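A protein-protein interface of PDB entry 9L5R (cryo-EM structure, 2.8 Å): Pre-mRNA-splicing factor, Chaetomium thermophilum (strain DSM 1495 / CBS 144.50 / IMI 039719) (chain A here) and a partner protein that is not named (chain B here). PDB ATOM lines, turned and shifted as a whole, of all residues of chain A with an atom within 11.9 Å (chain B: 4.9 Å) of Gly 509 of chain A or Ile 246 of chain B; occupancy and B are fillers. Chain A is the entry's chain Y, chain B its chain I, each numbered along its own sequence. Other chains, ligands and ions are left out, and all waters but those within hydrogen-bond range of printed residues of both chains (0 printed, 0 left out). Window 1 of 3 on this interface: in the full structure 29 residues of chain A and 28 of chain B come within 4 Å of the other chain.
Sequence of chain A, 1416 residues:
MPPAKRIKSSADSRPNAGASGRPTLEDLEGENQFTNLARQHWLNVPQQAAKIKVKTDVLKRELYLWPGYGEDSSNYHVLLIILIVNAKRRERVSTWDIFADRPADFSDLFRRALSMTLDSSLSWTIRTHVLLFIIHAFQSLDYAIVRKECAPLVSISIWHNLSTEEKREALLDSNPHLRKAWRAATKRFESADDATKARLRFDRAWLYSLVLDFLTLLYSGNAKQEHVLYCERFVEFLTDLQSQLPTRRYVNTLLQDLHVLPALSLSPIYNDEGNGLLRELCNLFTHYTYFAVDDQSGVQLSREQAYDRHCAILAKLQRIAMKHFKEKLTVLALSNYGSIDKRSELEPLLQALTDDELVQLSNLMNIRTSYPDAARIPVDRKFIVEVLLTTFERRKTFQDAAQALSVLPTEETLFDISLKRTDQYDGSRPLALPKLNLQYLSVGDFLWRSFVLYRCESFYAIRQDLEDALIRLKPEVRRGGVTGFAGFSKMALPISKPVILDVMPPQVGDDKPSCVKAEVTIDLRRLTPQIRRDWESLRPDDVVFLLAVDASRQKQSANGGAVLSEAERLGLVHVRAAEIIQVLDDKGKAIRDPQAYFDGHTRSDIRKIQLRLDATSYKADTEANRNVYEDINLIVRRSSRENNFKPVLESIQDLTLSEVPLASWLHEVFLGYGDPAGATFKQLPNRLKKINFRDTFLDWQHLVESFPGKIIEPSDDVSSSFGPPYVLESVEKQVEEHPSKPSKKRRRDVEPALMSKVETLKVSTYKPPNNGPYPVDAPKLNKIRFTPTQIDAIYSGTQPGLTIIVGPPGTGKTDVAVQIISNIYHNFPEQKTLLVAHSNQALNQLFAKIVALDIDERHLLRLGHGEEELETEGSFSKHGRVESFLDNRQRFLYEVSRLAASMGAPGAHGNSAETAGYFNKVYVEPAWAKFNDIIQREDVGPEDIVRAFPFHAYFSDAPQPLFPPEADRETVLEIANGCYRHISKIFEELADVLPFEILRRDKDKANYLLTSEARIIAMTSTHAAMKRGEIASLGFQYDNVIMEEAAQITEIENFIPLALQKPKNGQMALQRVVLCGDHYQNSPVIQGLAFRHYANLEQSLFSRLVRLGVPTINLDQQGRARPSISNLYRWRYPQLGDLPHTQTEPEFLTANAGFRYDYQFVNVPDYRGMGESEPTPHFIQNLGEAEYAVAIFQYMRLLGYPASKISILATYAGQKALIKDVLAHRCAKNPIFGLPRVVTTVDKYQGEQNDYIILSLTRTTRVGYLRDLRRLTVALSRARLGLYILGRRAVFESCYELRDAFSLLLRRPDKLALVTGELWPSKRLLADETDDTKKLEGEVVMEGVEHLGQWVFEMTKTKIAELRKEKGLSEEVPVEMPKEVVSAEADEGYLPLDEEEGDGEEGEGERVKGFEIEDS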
ATOM      1  N   ARG A 303      -3.225  10.247 -11.044  1.00  0.00           N
ATOM      2  CA  ARG A 303      -4.559   9.913 -10.550  1.00  0.00           C
ATOM      3  C   ARG A 303      -4.655  10.094  -9.042  1.00  0.00           C
ATOM      4  O   ARG A 303      -5.667  10.595  -8.535  1.00  0.00           O
ATOM      5  CB  ARG A 303      -4.905   8.474 -10.926  1.00  0.00           C
ATOM      6  CG  ARG A 303      -5.157   8.240 -12.404  1.00  0.00           C
ATOM      7  CD  ARG A 303      -5.324   6.755 -12.678  1.00  0.00           C
ATOM      8  NE  ARG A 303      -5.713   6.480 -14.055  1.00  0.00           N
ATOM      9  CZ  ARG A 303      -5.735   5.269 -14.596  1.00  0.00           C
ATOM     10  NH1 ARG A 303      -5.399   4.194 -13.901  1.00  0.00           N
ATOM     11  NH2 ARG A 303      -6.109   5.132 -15.865  1.00  0.00           N
ATOM     12  N   GLN A 403      -7.097   4.983 -22.077  1.00  0.00           N
ATOM     13  CA  GLN A 403      -7.483   3.612 -21.758  1.00  0.00           C
ATOM     14  C   GLN A 403      -8.872   3.291 -22.297  1.00  0.00           C
ATOM     15  O   GLN A 403      -9.124   2.170 -22.752  1.00  0.00           O
ATOM     16  CB  GLN A 403      -7.425   3.393 -20.247  1.00  0.00           C
ATOM     17  CG  GLN A 403      -7.115   1.964 -19.840  1.00  0.00           C
ATOM     18  CD  GLN A 403      -6.795   1.837 -18.364  1.00  0.00           C
ATOM     19  OE1 GLN A 403      -5.740   2.278 -17.907  1.00  0.00           O
ATOM     20  NE2 GLN A 403      -7.704   1.229 -17.611  1.00  0.00           N
ATOM     21  N   MET A 504     -10.042 -19.296 -26.368  1.00  0.00           N
ATOM     22  CA  MET A 504      -9.344 -19.637 -25.142  1.00  0.00           C
ATOM     23  C   MET A 504      -9.630 -18.570 -24.079  1.00  0.00           C
ATOM     24  O   MET A 504      -9.923 -17.421 -24.421  1.00  0.00           O
ATOM     25  CB  MET A 504      -7.844 -19.806 -25.431  1.00  0.00           C
ATOM     26  CG  MET A 504      -7.080 -18.599 -25.977  1.00  0.00           C
ATOM     27  SD  MET A 504      -6.584 -17.345 -24.785  1.00  0.00           S
ATOM     28  CE  MET A 504      -5.300 -18.217 -23.891  1.00  0.00           C
ATOM     29  N   PRO A 505      -9.600 -18.941 -22.789  1.00  0.00           N
ATOM     30  CA  PRO A 505     -10.112 -18.035 -21.755  1.00  0.00           C
ATOM     31  C   PRO A 505      -9.278 -16.772 -21.645  1.00  0.00           C
ATOM     32  O   PRO A 505      -8.074 -16.776 -21.950  1.00  0.00           O
ATOM     33  CB  PRO A 505     -10.023 -18.880 -20.470  1.00  0.00           C
ATOM     34  CG  PRO A 505      -9.016 -19.929 -20.775  1.00  0.00           C
ATOM     35  CD  PRO A 505      -9.240 -20.250 -22.216  1.00  0.00           C
ATOM     36  N   PRO A 506      -9.881 -15.659 -21.226  1.00  0.00           N
ATOM     37  CA  PRO A 506      -9.173 -14.374 -21.238  1.00  0.00           C
ATOM     38  C   PRO A 506      -8.064 -14.302 -20.200  1.00  0.00           C
ATOM     39  O   PRO A 506      -7.863 -15.208 -19.387  1.00  0.00           O
ATOM     40  CB  PRO A 506     -10.275 -13.356 -20.922  1.00  0.00           C
ATOM     41  CG  PRO A 506     -11.356 -14.145 -20.270  1.00  0.00           C
ATOM     42  CD  PRO A 506     -11.309 -15.496 -20.903  1.00  0.00           C
ATOM     43  N   GLN A 507      -7.339 -13.187 -20.244  1.00  0.00           N
ATOM     44  CA  GLN A 507      -6.273 -12.944 -19.288  1.00  0.00           C
ATOM     45  C   GLN A 507      -6.847 -12.687 -17.900  1.00  0.00           C
ATOM     46  O   GLN A 507      -8.034 -12.398 -17.725  1.00  0.00           O
ATOM     47  CB  GLN A 507      -5.415 -11.754 -19.718  1.00  0.00           C
ATOM     48  CG  GLN A 507      -4.877 -11.839 -21.130  1.00  0.00           C
ATOM     49  CD  GLN A 507      -3.935 -10.701 -21.464  1.00  0.00           C
ATOM     50  OE1 GLN A 507      -4.123  -9.571 -21.011  1.00  0.00           O
ATOM     51  NE2 GLN A 507      -2.913 -10.992 -22.260  1.00  0.00           N
ATOM     52  N   VAL A 508      -5.978 -12.803 -16.901  1.00  0.00           N
ATOM     53  CA  VAL A 508      -6.369 -12.583 -15.516  1.00  0.00           C
ATOM     54  C   VAL A 508      -6.135 -11.119 -15.170  1.00  0.00           C
ATOM     55  O   VAL A 508      -5.022 -10.723 -14.807  1.00  0.00           O
ATOM     56  CB  VAL A 508      -5.598 -13.529 -14.579  1.00  0.00           C
ATOM     57  CG1 VAL A 508      -6.140 -13.449 -13.175  1.00  0.00           C
ATOM     58  CG2 VAL A 508      -5.702 -14.948 -15.094  1.00  0.00           C
ATOM     59  N   GLY A 509      -7.184 -10.307 -15.284  1.00  0.00           N
ATOM     60  CA  GLY A 509      -7.067  -8.881 -15.054  1.00  0.00           C
ATOM     61  C   GLY A 509      -7.897  -8.036 -15.998  1.00  0.00           C
ATOM     62  O   GLY A 509      -7.901  -6.806 -15.892  1.00  0.00           O
ATOM     63  N   ASP A 510      -8.600  -8.677 -16.928  1.00  0.00           N
ATOM     64  CA  ASP A 510      -9.444  -7.959 -17.871  1.00  0.00           C
ATOM     65  C   ASP A 510     -10.680  -8.793 -18.175  1.00  0.00           C
ATOM     66  O   ASP A 510     -10.726  -9.998 -17.909  1.00  0.00           O
ATOM     67  CB  ASP A 510      -8.684  -7.614 -19.160  1.00  0.00           C
ATOM     68  CG  ASP A 510      -8.051  -8.829 -19.811  1.00  0.00           C
ATOM     69  OD1 ASP A 510      -8.029  -9.906 -19.181  1.00  0.00           O
ATOM     70  OD2 ASP A 510      -7.576  -8.706 -20.959  1.00  0.00           O
ATOM     71  N   ASP A 511     -11.689  -8.132 -18.740  1.00  0.00           N
ATOM     72  CA  ASP A 511     -12.936  -8.781 -19.122  1.00  0.00           C
ATOM     73  C   ASP A 511     -12.998  -9.160 -20.592  1.00  0.00           C
ATOM     74  O   ASP A 511     -13.713 -10.102 -20.942  1.00  0.00           O
ATOM     75  CB  ASP A 511     -14.128  -7.872 -18.795  1.00  0.00           C
ATOM     76  CG  ASP A 511     -13.914  -6.444 -19.253  1.00  0.00           C
ATOM     77  OD1 ASP A 511     -12.786  -6.118 -19.682  1.00  0.00           O
ATOM     78  OD2 ASP A 511     -14.871  -5.646 -19.185  1.00  0.00           O
ATOM     79  N   LYS A 512     -12.279  -8.447 -21.455  1.00  0.00           N
ATOM     80  CA  LYS A 512     -12.236  -8.792 -22.865  1.00  0.00           C
ATOM     81  C   LYS A 512     -11.474 -10.103 -23.065  1.00  0.00           C
ATOM     82  O   LYS A 512     -10.546 -10.407 -22.310  1.00  0.00           O
ATOM     83  CB  LYS A 512     -11.571  -7.673 -23.664  1.00  0.00           C
ATOM     84  CG  LYS A 512     -10.356  -7.069 -22.979  1.00  0.00           C
ATOM     85  CD  LYS A 512      -9.760  -5.939 -23.801  1.00  0.00           C
ATOM     86  CE  LYS A 512      -8.879  -6.475 -24.916  1.00  0.00           C
ATOM     87  NZ  LYS A 512      -7.773  -7.323 -24.391  1.00  0.00           N
ATOM     88  N   PRO A 513     -11.865 -10.906 -24.059  1.00  0.00           N
ATOM     89  CA  PRO A 513     -11.160 -12.170 -24.309  1.00  0.00           C
ATOM     90  C   PRO A 513      -9.721 -11.941 -24.747  1.00  0.00           C
ATOM     91  O   PRO A 513      -9.397 -10.957 -25.413  1.00  0.00           O
ATOM     92  CB  PRO A 513     -11.984 -12.825 -25.425  1.00  0.00           C
ATOM     93  CG  PRO A 513     -13.321 -12.164 -25.357  1.00  0.00           C
ATOM     94  CD  PRO A 513     -13.052 -10.760 -24.918  1.00  0.00           C
ATOM     95  N   SER A 514      -8.847 -12.864 -24.346  1.00  0.00           N
ATOM     96  CA  SER A 514      -7.435 -12.732 -24.691  1.00  0.00           C
ATOM     97  C   SER A 514      -7.181 -13.073 -26.154  1.00  0.00           C
ATOM     98  O   SER A 514      -6.402 -12.389 -26.828  1.00  0.00           O
ATOM     99  CB  SER A 514      -6.591 -13.615 -23.776  1.00  0.00           C
ATOM    100  OG  SER A 514      -6.954 -14.973 -23.910  1.00  0.00           O
ATOM    101  N   ALA A 615     -11.079  -8.225 -29.781  1.00  0.00           N
ATOM    102  CA  ALA A 615     -11.554  -8.733 -28.499  1.00  0.00           C
ATOM    103  C   ALA A 615     -12.749  -7.938 -27.992  1.00  0.00           C
ATOM    104  O   ALA A 615     -13.754  -8.517 -27.559  1.00  0.00           O
ATOM    105  CB  ALA A 615     -10.419  -8.702 -27.479  1.00  0.00           C
ATOM    106  N   LYS A 619     -16.548  -9.311 -27.667  1.00  0.00           N
ATOM    107  CA  LYS A 619     -17.258  -9.247 -26.394  1.00  0.00           C
ATOM    108  C   LYS A 619     -18.557  -8.459 -26.520  1.00  0.00           C
ATOM    109  O   LYS A 619     -19.577  -8.836 -25.928  1.00  0.00           O
ATOM    110  CB  LYS A 619     -16.356  -8.632 -25.324  1.00  0.00           C
ATOM    111  CG  LYS A 619     -16.876  -8.787 -23.905  1.00  0.00           C
ATOM    112  CD  LYS A 619     -16.281  -7.735 -22.984  1.00  0.00           C
ATOM    113  CE  LYS A 619     -16.937  -7.770 -21.614  1.00  0.00           C
ATOM    114  NZ  LYS A 619     -16.745  -6.491 -20.876  1.00  0.00           N
ATOM    115  N   LEU A 657      -0.105   5.845 -20.606  1.00  0.00           N
ATOM    116  CA  LEU A 657      -0.165   5.178 -19.310  1.00  0.00           C
ATOM    117  C   LEU A 657       1.132   5.354 -18.528  1.00  0.00           C
ATOM    118  O   LEU A 657       1.115   5.356 -17.292  1.00  0.00           O
ATOM    119  CB  LEU A 657      -0.491   3.694 -19.492  1.00  0.00           C
ATOM    120  CG  LEU A 657      -1.968   3.274 -19.444  1.00  0.00           C
ATOM    121  CD1 LEU A 657      -2.563   3.576 -18.075  1.00  0.00           C
ATOM    122  CD2 LEU A 657      -2.806   3.915 -20.545  1.00  0.00           C
ATOM    123  N   TRP B 219      -5.877 -17.615  -6.297  1.00  0.00           N
ATOM    124  CA  TRP B 219      -6.481 -16.301  -6.068  1.00  0.00           C
ATOM    125  C   TRP B 219      -6.360 -15.885  -4.607  1.00  0.00           C
ATOM    126  O   TRP B 219      -6.095 -14.713  -4.301  1.00  0.00           O
ATOM    127  CB  TRP B 219      -7.945 -16.315  -6.498  1.00  0.00           C
ATOM    128  CG  TRP B 219      -8.145 -15.893  -7.914  1.00  0.00           C
ATOM    129  CD1 TRP B 219      -8.229 -16.705  -9.004  1.00  0.00           C
ATOM    130  CD2 TRP B 219      -8.266 -14.553  -8.401  1.00  0.00           C
ATOM    131  NE1 TRP B 219      -8.408 -15.956 -10.140  1.00  0.00           N
ATOM    132  CE2 TRP B 219      -8.432 -14.631  -9.797  1.00  0.00           C
ATOM    133  CE3 TRP B 219      -8.254 -13.294  -7.792  1.00  0.00           C
ATOM    134  CZ2 TRP B 219      -8.588 -13.502 -10.593  1.00  0.00           C
ATOM    135  CZ3 TRP B 219      -8.406 -12.173  -8.586  1.00  0.00           C
ATOM    136  CH2 TRP B 219      -8.567 -12.286  -9.972  1.00  0.00           C
ATOM    137  N   ASP B 242      -2.587  -3.582 -11.042  1.00  0.00           N
ATOM    138  CA  ASP B 242      -3.799  -2.808 -10.770  1.00  0.00           C
ATOM    139  C   ASP B 242      -4.677  -3.640  -9.837  1.00  0.00           C
ATOM    140  O   ASP B 242      -5.407  -4.530 -10.287  1.00  0.00           O
ATOM    141  CB  ASP B 242      -4.514  -2.431 -12.067  1.00  0.00           C
ATOM    142  CG  ASP B 242      -4.571  -3.577 -13.065  1.00  0.00           C
ATOM    143  OD1 ASP B 242      -3.993  -4.647 -12.784  1.00  0.00           O
ATOM    144  OD2 ASP B 242      -5.181  -3.398 -14.140  1.00  0.00           O
ATOM    145  N   VAL B 243      -4.588  -3.346  -8.536  1.00  0.00           N
ATOM    146  CA  VAL B 243      -5.225  -4.179  -7.518  1.00  0.00           C
ATOM    147  C   VAL B 243      -6.743  -4.110  -7.627  1.00  0.00           C
ATOM    148  O   VAL B 243      -7.431  -5.135  -7.528  1.00  0.00           O
ATOM    149  CB  VAL B 243      -4.739  -3.774  -6.115  1.00  0.00           C
ATOM    150  CG1 VAL B 243      -5.216  -4.781  -5.079  1.00  0.00           C
ATOM    151  CG2 VAL B 243      -3.224  -3.654  -6.094  1.00  0.00           C
ATOM    152  N   GLU B 244      -7.286  -2.906  -7.834  1.00  0.00           N
ATOM    153  CA  GLU B 244      -8.729  -2.750  -7.991  1.00  0.00           C
ATOM    154  C   GLU B 244      -9.239  -3.517  -9.203  1.00  0.00           C
ATOM    155  O   GLU B 244     -10.262  -4.208  -9.125  1.00  0.00           O
ATOM    156  CB  GLU B 244      -9.084  -1.268  -8.111  1.00  0.00           C
ATOM    157  CG  GLU B 244      -9.100  -0.518  -6.792  1.00  0.00           C
ATOM    158  CD  GLU B 244     -10.372  -0.754  -6.004  1.00  0.00           C
ATOM    159  OE1 GLU B 244     -11.423  -1.003  -6.630  1.00  0.00           O
ATOM    160  OE2 GLU B 244     -10.321  -0.690  -4.759  1.00  0.00           O
ATOM    161  N   ARG B 245      -8.512  -3.441 -10.322  1.00  0.00           N
ATOM    162  CA  ARG B 245      -8.949  -4.115 -11.539  1.00  0.00           C
ATOM    163  C   ARG B 245      -8.857  -5.632 -11.408  1.00  0.00           C
ATOM    164  O   ARG B 245      -9.766  -6.346 -11.846  1.00  0.00           O
ATOM    165  CB  ARG B 245      -8.132  -3.628 -12.733  1.00  0.00           C
ATOM    166  CG  ARG B 245      -8.645  -4.138 -14.066  1.00  0.00           C
ATOM    167  CD  ARG B 245     -10.065  -3.657 -14.310  1.00  0.00           C
ATOM    168  NE  ARG B 245     -10.681  -4.307 -15.460  1.00  0.00           N
ATOM    169  CZ  ARG B 245     -11.318  -5.468 -15.410  1.00  0.00           C
ATOM    170  NH1 ARG B 245     -11.431  -6.147 -14.280  1.00  0.00           N
ATOM    171  NH2 ARG B 245     -11.859  -5.960 -16.521  1.00  0.00           N
ATOM    172  N   ILE B 246      -7.780  -6.146 -10.804  1.00  0.00           N
ATOM    173  CA  ILE B 246      -7.649  -7.597 -10.675  1.00  0.00           C
ATOM    174  C   ILE B 246      -8.672  -8.146  -9.681  1.00  0.00           C
ATOM    175  O   ILE B 246      -9.250  -9.219  -9.900  1.00  0.00           O
ATOM    176  CB  ILE B 246      -6.199  -8.000 -10.321  1.00  0.00           C
ATOM    177  CG1 ILE B 246      -6.040  -9.519 -10.355  1.00  0.00           C
ATOM    178  CG2 ILE B 246      -5.753  -7.500  -8.963  1.00  0.00           C
ATOM    179  CD1 ILE B 246      -6.202 -10.101 -11.715  1.00  0.00           C
ATOM    180  N   ILE B 247      -8.960  -7.406  -8.607  1.00  0.00           N
ATOM    181  CA  ILE B 247      -9.948  -7.897  -7.656  1.00  0.00           C
ATOM    182  C   ILE B 247     -11.362  -7.786  -8.230  1.00  0.00           C
ATOM    183  O   ILE B 247     -12.196  -8.661  -7.986  1.00  0.00           O
ATOM    184  CB  ILE B 247      -9.774  -7.179  -6.305  1.00  0.00           C
ATOM    185  CG1 ILE B 247      -8.441  -7.614  -5.688  1.00  0.00           C
ATOM    186  CG2 ILE B 247     -10.912  -7.496  -5.342  1.00  0.00           C
ATOM    187  CD1 ILE B 247      -8.202  -7.146  -4.276  1.00  0.00           C
ATOM    188  N   ARG B 248     -11.647  -6.770  -9.052  1.00  0.00           N
ATOM    189  CA  ARG B 248     -12.946  -6.723  -9.722  1.00  0.00           C
ATOM    190  C   ARG B 248     -13.076  -7.807 -10.790  1.00  0.00           C
ATOM    191  O   ARG B 248     -14.181  -8.317 -11.023  1.00  0.00           O
ATOM    192  CB  ARG B 248     -13.175  -5.339 -10.328  1.00  0.00           C
ATOM    193  CG  ARG B 248     -13.580  -4.292  -9.303  1.00  0.00           C
ATOM    194  CD  ARG B 248     -14.071  -3.016  -9.961  1.00  0.00           C
ATOM    195  NE  ARG B 248     -14.275  -1.952  -8.984  1.00  0.00           N
ATOM    196  CZ  ARG B 248     -14.830  -0.779  -9.256  1.00  0.00           C
ATOM    197  NH1 ARG B 248     -15.256  -0.482 -10.473  1.00  0.00           N
ATOM    198  NH2 ARG B 248     -14.964   0.117  -8.283  1.00  0.00           N
ATOM    199  N   SER B 249     -11.968  -8.171 -11.444  1.00  0.00           N
ATOM    200  CA  SER B 249     -11.979  -9.324 -12.339  1.00  0.00           C
ATOM    201  C   SER B 249     -12.283 -10.604 -11.573  1.00  0.00           C
ATOM    202  O   SER B 249     -13.047 -11.457 -12.043  1.00  0.00           O
ATOM    203  CB  SER B 249     -10.641  -9.435 -13.069  1.00  0.00           C
ATOM    204  OG  SER B 249     -10.427 -10.754 -13.542  1.00  0.00           O
ATOM    205  N   GLY B 250     -11.702 -10.748 -10.380  1.00  0.00           N
ATOM    206  CA  GLY B 250     -12.067 -11.858  -9.515  1.00  0.00           C
ATOM    207  C   GLY B 250     -13.516 -11.816  -9.069  1.00  0.00           C
ATOM    208  O   GLY B 250     -14.138 -12.863  -8.880  1.00  0.00           O
ATOM    209  N   ARG B 253     -15.515 -13.011 -12.006  1.00  0.00           N
ATOM    210  CA  ARG B 253     -15.203 -14.394 -12.352  1.00  0.00           C
ATOM    211  C   ARG B 253     -15.677 -15.381 -11.289  1.00  0.00           C
ATOM    212  O   ARG B 253     -16.501 -16.256 -11.574  1.00  0.00           O
ATOM    213  CB  ARG B 253     -13.695 -14.540 -12.587  1.00  0.00           C
ATOM    214  CG  ARG B 253     -13.267 -15.913 -13.072  1.00  0.00           C
ATOM    215  CD  ARG B 253     -11.755 -16.008 -13.134  1.00  0.00           C
ATOM    216  NE  ARG B 253     -11.195 -14.942 -13.956  1.00  0.00           N
ATOM    217  CZ  ARG B 253      -9.899 -14.747 -14.155  1.00  0.00           C
ATOM    218  NH1 ARG B 253      -8.989 -15.530 -13.599  1.00  0.00           N
ATOM    219  NH2 ARG B 253      -9.507 -13.740 -14.929  1.00  0.00           N
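NH2 of Arg 245 of chain B is in salt-bridge range of OD1 of Asp 511 of chain A.
O of Gln 507 of chain A is in hydrogen-bond range of NH2 of Arg 253 of chain B (3.4 Å).
The guanidinium group of Arg 253 of chain B is in hydrogen-bond range of the side-chain hydroxyl of Ser 249 of chain B (3.4 Å).
NZ of Lys 512 of chain A is in salt-bridge range of OD2 of Asp 510 of chain A (3.7 Å).
NZ of Lys 619 of chain A is in salt-bridge range of OD2 of Asp 511 of chain A, 2.7 Å away.
Among the printed residues, merely in contact across the chains: Gly 509 of chain A with Arg 245 of chain B (3.3 Å), Val 508 of chain A with Ile 246 of chain B (3.4 Å), Val 508 of chain A with Arg 253 of chain B (3.4 Å), Asp 510 of chain A with Arg 245 of chain B (3.4 Å), Val 508 of chain A with Trp 219 of chain B (3.6 Å), Gly 509 of chain A with Ile 246 of chain B (3.7 Å) and Gly 509 of chain A with Ser 249 of chain B (3.7 Å).
Gly 509 of chain A touches just these residues of chain B: Arg 245 (3.3 Å), Ile 246 (3.7 Å) and Ser 249 (3.7 Å).
Ile 246 of chain B touches just these residues of chain A: Val 508 (3.4 Å) and Gly 509 (3.7 Å).
No residue of chain A comes within 4 Å of Asp 242 of chain B.
No residue of chain A comes within 4 Å of Val 243 of chain B.
Arg 245 of chain B touches three residues of chain A.
Gly 250 of chain B touches none of the printed residues of chain A.
Printed residues of chain B within 4 Å of Asp 510 of chain A: Arg 245 (3.4 Å).
Of the printed residues of chain B, Val 508 of chain A touches Trp 219, Ile 246 and Arg 253.
Printed residues of chain B within 4 Å of Asp 511 of chain A: Arg 245.
Of the printed residues of chain A, Arg 253 of chain B touches Gln 507 and Val 508.
Of the printed residues of chain B, Gln 507 of chain A touches Arg 253 (3.4 Å).
The nearest residue of chain B that does not touch Gly 509 of chain A is Arg 253 of chain B (4.2 Å).
The nearest residue of chain A that does not touch Ile 246 of chain B is Asp 510 of chain A (5.9 Å).
Printed residues of chain B that touch a printed residue of chain A: Trp 219, Arg 245, Ile 246, Ser 249 and Arg 253.
Of the 16 printed residues of chain A, 5 touch a printed residue of chain B.
Hydrophobic or aromatic side chains of chain A that line the printed part of chain B: Val 508.
Among the printed residues, Asp or Glu carboxylates within 4 Å of a Lys or Arg side-chain nitrogen of the other chain: Asp 511 of chain A with Arg 245 of chain B.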
